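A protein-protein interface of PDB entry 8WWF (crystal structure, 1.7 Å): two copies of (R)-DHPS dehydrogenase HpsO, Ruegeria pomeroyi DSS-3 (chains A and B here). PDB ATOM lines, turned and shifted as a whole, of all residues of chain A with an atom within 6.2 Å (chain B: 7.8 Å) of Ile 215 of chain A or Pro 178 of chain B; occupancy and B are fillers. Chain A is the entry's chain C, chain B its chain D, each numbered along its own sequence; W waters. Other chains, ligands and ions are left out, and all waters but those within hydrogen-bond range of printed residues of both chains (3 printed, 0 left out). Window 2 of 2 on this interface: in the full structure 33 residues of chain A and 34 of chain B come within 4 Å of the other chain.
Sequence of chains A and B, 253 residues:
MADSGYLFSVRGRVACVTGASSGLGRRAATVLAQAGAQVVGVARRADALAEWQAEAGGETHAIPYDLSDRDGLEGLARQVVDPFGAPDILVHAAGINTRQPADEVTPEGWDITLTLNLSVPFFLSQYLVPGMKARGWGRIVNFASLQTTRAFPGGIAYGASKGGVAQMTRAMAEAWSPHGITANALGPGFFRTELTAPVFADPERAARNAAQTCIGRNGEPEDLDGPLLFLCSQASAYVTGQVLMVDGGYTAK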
ATOM      1  N   ALA A 210      -3.888 -21.433  -3.888  1.00  0.00           N
ATOM      2  CA  ALA A 210      -4.310 -21.156  -5.277  1.00  0.00           C
ATOM      3  C   ALA A 210      -4.721 -22.427  -5.997  1.00  0.00           C
ATOM      4  O   ALA A 210      -5.744 -22.454  -6.718  1.00  0.00           O
ATOM      5  CB  ALA A 210      -3.174 -20.412  -6.013  1.00  0.00           C
ATOM      6  N   THR A 213      -8.277 -23.861  -5.539  1.00  0.00           N
ATOM      7  CA  THR A 213      -9.400 -23.324  -6.223  1.00  0.00           C
ATOM      8  C   THR A 213      -9.562 -24.021  -7.591  1.00  0.00           C
ATOM      9  O   THR A 213      -8.725 -24.840  -8.053  1.00  0.00           O
ATOM     10  CB  THR A 213      -9.201 -21.822  -6.505  1.00  0.00           C
ATOM     11  OG1 THR A 213      -8.159 -21.678  -7.483  1.00  0.00           O
ATOM     12  CG2 THR A 213      -8.911 -21.050  -5.207  1.00  0.00           C
ATOM     13  N   CYS A 214     -10.753 -23.863  -8.207  1.00  0.00           N
ATOM     14  CA  CYS A 214     -10.979 -24.393  -9.554  1.00  0.00           C
ATOM     15  C   CYS A 214     -10.237 -23.615 -10.630  1.00  0.00           C
ATOM     16  O   CYS A 214      -9.794 -24.186 -11.616  1.00  0.00           O
ATOM     17  CB  CYS A 214     -12.467 -24.410  -9.862  1.00  0.00           C
ATOM     18  SG  CYS A 214     -13.437 -25.635  -8.878  1.00  0.00           S
ATOM     19  N   ILE A 215     -10.143 -22.297 -10.450  1.00  0.00           N
ATOM     20  CA  ILE A 215      -9.490 -21.450 -11.437  1.00  0.00           C
ATOM     21  C   ILE A 215      -7.968 -21.628 -11.376  1.00  0.00           C
ATOM     22  O   ILE A 215      -7.305 -21.591 -12.450  1.00  0.00           O
ATOM     23  CB  ILE A 215      -9.869 -19.989 -11.204  1.00  0.00           C
ATOM     24  CG1 ILE A 215     -11.361 -19.830 -11.384  1.00  0.00           C
ATOM     25  CG2 ILE A 215      -9.069 -19.094 -12.159  1.00  0.00           C
ATOM     26  CD1 ILE A 215     -11.840 -18.402 -11.190  1.00  0.00           C
ATOM     27  N   GLY A 216      -7.416 -21.901 -10.176  1.00  0.00           N
ATOM     28  CA  GLY A 216      -6.021 -21.977 -10.010  1.00  0.00           C
ATOM     29  C   GLY A 216      -5.271 -20.726  -9.608  1.00  0.00           C
ATOM     30  O   GLY A 216      -4.029 -20.748  -9.697  1.00  0.00           O
ATOM     31  N   ARG A 217      -5.957 -19.714  -9.033  1.00  0.00           N
ATOM     32  CA  ARG A 217      -5.317 -18.520  -8.557  1.00  0.00           C
ATOM     33  C   ARG A 217      -6.012 -18.040  -7.334  1.00  0.00           C
ATOM     34  O   ARG A 217      -7.212 -18.326  -7.175  1.00  0.00           O
ATOM     35  CB  ARG A 217      -5.327 -17.394  -9.587  1.00  0.00           C
ATOM     36  CG  ARG A 217      -6.729 -16.894  -9.952  1.00  0.00           C
ATOM     37  CD  ARG A 217      -6.662 -15.771 -10.979  1.00  0.00           C
ATOM     38  NE  ARG A 217      -7.926 -15.209 -11.345  1.00  0.00           N
ATOM     39  CZ  ARG A 217      -8.613 -14.305 -10.618  1.00  0.00           C
ATOM     40  NH1 ARG A 217      -8.175 -13.902  -9.471  1.00  0.00           N
ATOM     41  NH2 ARG A 217      -9.762 -13.785 -11.081  1.00  0.00           N
ATOM     42  N   ASP A 247     -14.518 -17.188  -4.405  1.00  0.00           N
ATOM     43  CA  ASP A 247     -13.396 -17.993  -4.006  1.00  0.00           C
ATOM     44  C   ASP A 247     -12.740 -18.765  -5.096  1.00  0.00           C
ATOM     45  O   ASP A 247     -11.988 -19.715  -4.852  1.00  0.00           O
ATOM     46  CB  ASP A 247     -13.784 -18.926  -2.878  1.00  0.00           C
ATOM     47  CG  ASP A 247     -14.737 -20.042  -3.276  1.00  0.00           C
ATOM     48  OD1 ASP A 247     -15.112 -20.134  -4.447  1.00  0.00           O
ATOM     49  OD2 ASP A 247     -15.057 -20.875  -2.408  1.00  0.00           O
ATOM     50  N   GLY A 248     -13.061 -18.439  -6.359  1.00  0.00           N
ATOM     51  CA  GLY A 248     -12.555 -19.178  -7.471  1.00  0.00           C
ATOM     52  C   GLY A 248     -12.818 -20.628  -7.510  1.00  0.00           C
ATOM     53  O   GLY A 248     -12.186 -21.384  -8.197  1.00  0.00           O
ATOM     54  N   GLY A 249     -13.862 -21.014  -6.777  1.00  0.00           N
ATOM     55  CA  GLY A 249     -14.229 -22.424  -6.702  1.00  0.00           C
ATOM     56  C   GLY A 249     -13.516 -23.223  -5.628  1.00  0.00           C
ATOM     57  O   GLY A 249     -13.535 -24.478  -5.633  1.00  0.00           O
ATOM     58  N   LYS B 133     -12.948 -22.473 -24.637  1.00  0.00           N
ATOM     59  CA  LYS B 133     -11.541 -22.632 -24.327  1.00  0.00           C
ATOM     60  C   LYS B 133     -10.617 -21.915 -25.308  1.00  0.00           C
ATOM     61  O   LYS B 133      -9.590 -21.383 -24.898  1.00  0.00           O
ATOM     62  CB  LYS B 133     -11.190 -24.130 -24.333  1.00  0.00           C
ATOM     63  CG  LYS B 133     -11.758 -24.925 -23.185  1.00  0.00           C
ATOM     64  CD  LYS B 133     -11.214 -26.344 -23.214  1.00  0.00           C
ATOM     65  CE  LYS B 133     -11.726 -27.135 -22.059  1.00  0.00           C
ATOM     66  NZ  LYS B 133     -11.412 -28.555 -22.309  1.00  0.00           N
ATOM     67  N   GLY B 136     -10.407 -18.534 -24.171  1.00  0.00           N
ATOM     68  CA  GLY B 136     -10.068 -18.390 -22.803  1.00  0.00           C
ATOM     69  C   GLY B 136     -11.132 -17.754 -21.909  1.00  0.00           C
ATOM     70  O   GLY B 136     -10.799 -17.166 -20.908  1.00  0.00           O
ATOM     71  N   ALA B 171     -18.359 -29.798 -10.469  1.00  0.00           N
ATOM     72  CA  ALA B 171     -17.468 -30.599 -11.318  1.00  0.00           C
ATOM     73  C   ALA B 171     -17.140 -29.929 -12.634  1.00  0.00           C
ATOM     74  O   ALA B 171     -15.988 -30.004 -13.151  1.00  0.00           O
ATOM     75  CB  ALA B 171     -18.040 -31.993 -11.514  1.00  0.00           C
ATOM     76  N   MET B 172     -18.091 -29.207 -13.184  1.00  0.00           N
ATOM     77  CA  MET B 172     -17.834 -28.429 -14.427  1.00  0.00           C
ATOM     78  C   MET B 172     -16.769 -27.374 -14.112  1.00  0.00           C
ATOM     79  O   MET B 172     -15.827 -27.119 -14.906  1.00  0.00           O
ATOM     80  CB  MET B 172     -19.083 -27.732 -14.941  1.00  0.00           C
ATOM     81  CG  MET B 172     -19.998 -28.705 -15.659  1.00  0.00           C
ATOM     82  SD  MET B 172     -21.454 -27.920 -16.318  1.00  0.00           S
ATOM     83  CE  MET B 172     -22.098 -29.266 -17.348  1.00  0.00           C
ATOM     84  N   ALA B 173     -16.919 -26.711 -12.963  1.00  0.00           N
ATOM     85  CA  ALA B 173     -15.899 -25.768 -12.545  1.00  0.00           C
ATOM     86  C   ALA B 173     -14.555 -26.396 -12.353  1.00  0.00           C
ATOM     87  O   ALA B 173     -13.535 -25.912 -12.787  1.00  0.00           O
ATOM     88  CB  ALA B 173     -16.377 -24.969 -11.291  1.00  0.00           C
ATOM     89  N   GLU B 174     -14.495 -27.547 -11.739  1.00  0.00           N
ATOM     90  CA  GLU B 174     -13.214 -28.193 -11.501  1.00  0.00           C
ATOM     91  C   GLU B 174     -12.534 -28.593 -12.814  1.00  0.00           C
ATOM     92  O   GLU B 174     -11.301 -28.475 -12.933  1.00  0.00           O
ATOM     93  CB  GLU B 174     -13.463 -29.465 -10.643  1.00  0.00           C
ATOM     94  CG  GLU B 174     -12.178 -30.227 -10.198  1.00  0.00           C
ATOM     95  CD  GLU B 174     -11.536 -31.207 -11.204  1.00  0.00           C
ATOM     96  OE1 GLU B 174     -12.174 -31.667 -12.160  1.00  0.00           O
ATOM     97  OE2 GLU B 174     -10.314 -31.577 -11.015  1.00  0.00           O
ATOM     98  N   ALA B 175     -13.319 -28.980 -13.813  1.00  0.00           N
ATOM     99  CA  ALA B 175     -12.730 -29.418 -15.101  1.00  0.00           C
ATOM    100  C   ALA B 175     -12.345 -28.215 -15.998  1.00  0.00           C
ATOM    101  O   ALA B 175     -11.293 -28.277 -16.662  1.00  0.00           O
ATOM    102  CB  ALA B 175     -13.683 -30.344 -15.793  1.00  0.00           C
ATOM    103  N   TRP B 176     -13.198 -27.184 -16.011  1.00  0.00           N
ATOM    104  CA  TRP B 176     -13.153 -26.127 -16.993  1.00  0.00           C
ATOM    105  C   TRP B 176     -12.724 -24.775 -16.526  1.00  0.00           C
ATOM    106  O   TRP B 176     -12.285 -23.958 -17.357  1.00  0.00           O
ATOM    107  CB  TRP B 176     -14.526 -26.056 -17.703  1.00  0.00           C
ATOM    108  CG  TRP B 176     -14.820 -27.370 -18.456  1.00  0.00           C
ATOM    109  CD1 TRP B 176     -13.915 -28.157 -19.165  1.00  0.00           C
ATOM    110  CD2 TRP B 176     -16.108 -27.888 -18.749  1.00  0.00           C
ATOM    111  NE1 TRP B 176     -14.607 -29.223 -19.773  1.00  0.00           N
ATOM    112  CE2 TRP B 176     -15.935 -29.055 -19.559  1.00  0.00           C
ATOM    113  CE3 TRP B 176     -17.359 -27.518 -18.372  1.00  0.00           C
ATOM    114  CZ2 TRP B 176     -16.997 -29.848 -19.953  1.00  0.00           C
ATOM    115  CZ3 TRP B 176     -18.477 -28.278 -18.793  1.00  0.00           C
ATOM    116  CH2 TRP B 176     -18.260 -29.416 -19.631  1.00  0.00           C
ATOM    117  N   SER B 177     -12.888 -24.447 -15.232  1.00  0.00           N
ATOM    118  CA  SER B 177     -12.506 -23.162 -14.787  1.00  0.00           C
ATOM    119  C   SER B 177     -10.973 -22.843 -14.882  1.00  0.00           C
ATOM    120  O   SER B 177     -10.656 -21.661 -14.958  1.00  0.00           O
ATOM    121  CB  SER B 177     -13.042 -22.868 -13.398  1.00  0.00           C
ATOM    122  OG  SER B 177     -14.467 -22.789 -13.490  1.00  0.00           O
ATOM    123  N   PRO B 178     -10.099 -23.859 -14.995  1.00  0.00           N
ATOM    124  CA  PRO B 178      -8.690 -23.496 -15.286  1.00  0.00           C
ATOM    125  C   PRO B 178      -8.550 -22.868 -16.670  1.00  0.00           C
ATOM    126  O   PRO B 178      -7.510 -22.281 -16.907  1.00  0.00           O
ATOM    127  CB  PRO B 178      -7.961 -24.811 -15.208  1.00  0.00           C
ATOM    128  CG  PRO B 178      -8.770 -25.628 -14.256  1.00  0.00           C
ATOM    129  CD  PRO B 178     -10.157 -25.278 -14.544  1.00  0.00           C
ATOM    130  N   HIS B 179      -9.559 -22.967 -17.505  1.00  0.00           N
ATOM    131  CA  HIS B 179      -9.475 -22.548 -18.887  1.00  0.00           C
ATOM    132  C   HIS B 179     -10.269 -21.314 -19.165  1.00  0.00           C
ATOM    133  O   HIS B 179     -10.519 -20.911 -20.323  1.00  0.00           O
ATOM    134  CB  HIS B 179      -9.859 -23.800 -19.805  1.00  0.00           C
ATOM    135  CG  HIS B 179      -9.095 -25.018 -19.478  1.00  0.00           C
ATOM    136  ND1 HIS B 179      -7.727 -25.117 -19.670  1.00  0.00           N
ATOM    137  CD2 HIS B 179      -9.461 -26.145 -18.825  1.00  0.00           C
ATOM    138  CE1 HIS B 179      -7.294 -26.257 -19.168  1.00  0.00           C
ATOM    139  NE2 HIS B 179      -8.325 -26.902 -18.650  1.00  0.00           N
ATOM    140  N   GLY B 180     -10.692 -20.639 -18.132  1.00  0.00           N
ATOM    141  CA  GLY B 180     -11.417 -19.420 -18.270  1.00  0.00           C
ATOM    142  C   GLY B 180     -12.948 -19.535 -18.246  1.00  0.00           C
ATOM    143  O   GLY B 180     -13.626 -18.566 -18.386  1.00  0.00           O
ATOM    144  N   ILE B 181     -13.451 -20.755 -18.116  1.00  0.00           N
ATOM    145  CA  ILE B 181     -14.896 -20.975 -18.153  1.00  0.00           C
ATOM    146  C   ILE B 181     -15.417 -21.132 -16.752  1.00  0.00           C
ATOM    147  O   ILE B 181     -15.036 -22.142 -16.101  1.00  0.00           O
ATOM    148  CB  ILE B 181     -15.205 -22.233 -18.929  1.00  0.00           C
ATOM    149  CG1 ILE B 181     -14.680 -22.141 -20.398  1.00  0.00           C
ATOM    150  CG2 ILE B 181     -16.729 -22.542 -18.894  1.00  0.00           C
ATOM    151  CD1 ILE B 181     -14.429 -23.489 -20.965  1.00  0.00           C
ATOM    152  N   THR B 182     -16.321 -20.272 -16.280  1.00  0.00           N
ATOM    153  CA  THR B 182     -16.928 -20.503 -14.992  1.00  0.00           C
ATOM    154  C   THR B 182     -18.240 -21.228 -15.181  1.00  0.00           C
ATOM    155  O   THR B 182     -18.835 -21.200 -16.258  1.00  0.00           O
ATOM    156  CB  THR B 182     -17.203 -19.138 -14.292  1.00  0.00           C
ATOM    157  OG1 THR B 182     -18.169 -18.409 -15.044  1.00  0.00           O
ATOM    158  CG2 THR B 182     -15.876 -18.339 -13.962  1.00  0.00           C
ATOM    159  N   SER B 236     -18.575 -11.777 -12.468  1.00  0.00           N
ATOM    160  CA  SER B 236     -18.523 -13.000 -11.705  1.00  0.00           C
ATOM    161  C   SER B 236     -17.273 -13.809 -12.022  1.00  0.00           C
ATOM    162  O   SER B 236     -17.235 -15.012 -11.837  1.00  0.00           O
ATOM    163  CB  SER B 236     -19.830 -13.837 -11.976  1.00  0.00           C
ATOM    164  OG  SER B 236     -20.030 -14.156 -13.363  1.00  0.00           O
ATOM    165  N   ALA B 237     -16.225 -13.186 -12.585  1.00  0.00           N
ATOM    166  CA  ALA B 237     -15.023 -13.951 -12.961  1.00  0.00           C
ATOM    167  C   ALA B 237     -14.428 -14.855 -11.874  1.00  0.00           C
ATOM    168  O   ALA B 237     -13.893 -15.897 -12.193  1.00  0.00           O
ATOM    169  CB  ALA B 237     -13.921 -13.081 -13.471  1.00  0.00           C
ATOM    170  N   TYR B 238     -14.472 -14.427 -10.625  1.00  0.00           N
ATOM    171  CA  TYR B 238     -13.965 -15.208  -9.514  1.00  0.00           C
ATOM    172  C   TYR B 238     -15.035 -16.002  -8.750  1.00  0.00           C
ATOM    173  O   TYR B 238     -14.735 -16.476  -7.664  1.00  0.00           O
ATOM    174  CB  TYR B 238     -13.102 -14.344  -8.584  1.00  0.00           C
ATOM    175  CG  TYR B 238     -12.060 -15.098  -7.783  1.00  0.00           C
ATOM    176  CD1 TYR B 238     -11.113 -15.854  -8.458  1.00  0.00           C
ATOM    177  CD2 TYR B 238     -11.977 -15.057  -6.414  1.00  0.00           C
ATOM    178  CE1 TYR B 238     -10.126 -16.572  -7.777  1.00  0.00           C
ATOM    179  CE2 TYR B 238     -11.008 -15.774  -5.720  1.00  0.00           C
ATOM    180  CZ  TYR B 238     -10.089 -16.550  -6.405  1.00  0.00           C
ATOM    181  OH  TYR B 238      -9.167 -17.238  -5.678  1.00  0.00           O
ATOM    182  N   VAL B 239     -16.176 -16.158  -9.343  1.00  0.00           N
ATOM    183  CA  VAL B 239     -17.346 -16.939  -8.780  1.00  0.00           C
ATOM    184  C   VAL B 239     -17.502 -18.139  -9.704  1.00  0.00           C
ATOM    185  O   VAL B 239     -17.793 -18.014 -10.857  1.00  0.00           O
ATOM    186  CB  VAL B 239     -18.675 -16.127  -8.680  1.00  0.00           C
ATOM    187  CG1 VAL B 239     -19.770 -17.009  -8.153  1.00  0.00           C
ATOM    188  CG2 VAL B 239     -18.570 -14.913  -7.775  1.00  0.00           C
ATOM    189  N   THR B 240     -17.209 -19.329  -9.170  1.00  0.00           N
ATOM    190  CA  THR B 240     -17.336 -20.556  -9.965  1.00  0.00           C
ATOM    191  C   THR B 240     -17.581 -21.724  -9.053  1.00  0.00           C
ATOM    192  O   THR B 240     -17.156 -21.733  -7.904  1.00  0.00           O
ATOM    193  CB  THR B 240     -16.165 -20.801 -10.929  1.00  0.00           C
ATOM    194  OG1 THR B 240     -16.560 -21.763 -11.886  1.00  0.00           O
ATOM    195  CG2 THR B 240     -14.953 -21.247 -10.201  1.00  0.00           C
HETATM  196  O   HOH W   1      -9.582 -18.187  -2.937  1.00  0.00           O
HETATM  197  O   HOH W   2      -9.748 -27.145 -11.105  1.00  0.00           O
HETATM  198  O   HOH W   3     -16.852 -18.789  -6.039  1.00  0.00           O
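The backbone NH of Asp 247 of chain A lies within hydrogen-bond range of the backbone carbonyl oxygen of Tyr 238 of chain B, 3.3 Å away.
The backbone nitrogen (N) of Pro 178 of chain B sits close to the backbone carbonyl oxygen (O) of Cys 214 of chain A, at 3.4 Å.
The side-chain sulfur of Cys 214 of chain A lies within hydrogen-bond range of the backbone NH of Glu 174 of chain B, at 3.6 Å.
O of Arg 217 of chain A sits at hydrogen-bond distance from OH of Tyr 238 of chain B.
O of Tyr 238 of chain B is in hydrogen-bond range of N of Gly 248 of chain A (2.9 Å).
The side-chain carboxylate (OD1) of Asp 247 of chain A is in hydrogen-bond range of the backbone NH (N) of Gly 249 of chain A (2.8 Å).
The backbone carbonyl oxygen (O) of Ile 181 of chain B sits at hydrogen-bond distance from the side-chain hydroxyl (OG) of Ser 177 of chain B (2.7 Å).
N of Gly 216 of chain A is in hydrogen-bond range of OG1 of Thr 213 of chain A, 2.8 Å away.
O of Ala 210 of chain A is in hydrogen-bond range of OG1 of Thr 213 of chain A (2.6 Å).
N of Cys 214 of chain A sits at hydrogen-bond distance from O of Gly 248 of chain A.
N of Arg 217 of chain A is in hydrogen-bond range of OG1 of Thr 213 of chain A, at 3.3 Å.
Among the printed residues, merely in contact across the chains: Gly 249 of chain A with Thr 240 of chain B (3.2 Å), Ile 215 of chain A with Ala 237 of chain B (3.4 Å), Gly 248 of chain A with Thr 240 of chain B (3.4 Å), Cys 214 of chain A with Ala 173 of chain B (3.5 Å), Ile 215 of chain A with Pro 178 of chain B (3.7 Å), Ile 215 of chain A with Ser 177 of chain B (3.7 Å), Cys 214 of chain A with Ser 177 of chain B (3.7 Å), Ile 215 of chain A with Tyr 238 of chain B (3.8 Å) and Thr 213 of chain A with Tyr 238 of chain B (3.8 Å).
Printed residues of chain B within 4 Å of Ile 215 of chain A: Ser 177 (3.7 Å), Pro 178 (3.7 Å), Ala 237 (3.4 Å) and Tyr 238 (3.8 Å).
Pro 178 of chain B touches two residues of chain A.
Of the printed residues of chain A, Ser 177 of chain B touches Cys 214 (3.7 Å) and Ile 215 (3.7 Å).
Of the printed residues of chain B, Asp 247 of chain A touches Tyr 238.
Of the printed residues of chain B, Gly 249 of chain A touches Thr 240.
Ala 171 of chain B touches none of the printed residues of chain A.
Gly 216 of chain A touches none of the printed residues of chain B.
The nearest residue of chain B that does not touch Ile 215 of chain A is Thr 240 of chain B (4.04 Å).
The nearest printed residue of chain A that does not touch Thr 240 of chain B is Cys 214 of chain A (4.04 Å).
Of the 9 printed residues of chain A, 7 touch a printed residue of chain B.
Hydrophobic or aromatic side chains of chain A that line the printed part of chain B: Ile 215.
Hydrophobic or aromatic side chains of chain B within 4 Å of the printed part of chain A: Ala 173, Pro 178 and Tyr 238.
Among the printed residues, 14 pairs touch across the chains.
Among the printed residues, no Asp or Glu carboxylate lies within 4 Å of a Lys or Arg side-chain nitrogen of the other chain.
No position is printed for both chains.
Of the 14 pairs that touch across the chains among the printed residues, none has its exchanged pair printed and touching as well.
Water W3 bridges the side-chain carboxylate (OD1) of Asp 247 of chain A (2.7 Å) and the backbone NH (N) of Thr 240 of chain B (3.2 Å).
Water W2 lies within hydrogen-bond range of O of Glu 174 of chain B (2.7 Å) and O of Cys 214 of chain A (3.0 Å).
Water W1 bridges OH of Tyr 238 of chain B (2.9 Å) and O of Asp 247 of chain A (3.4 Å).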
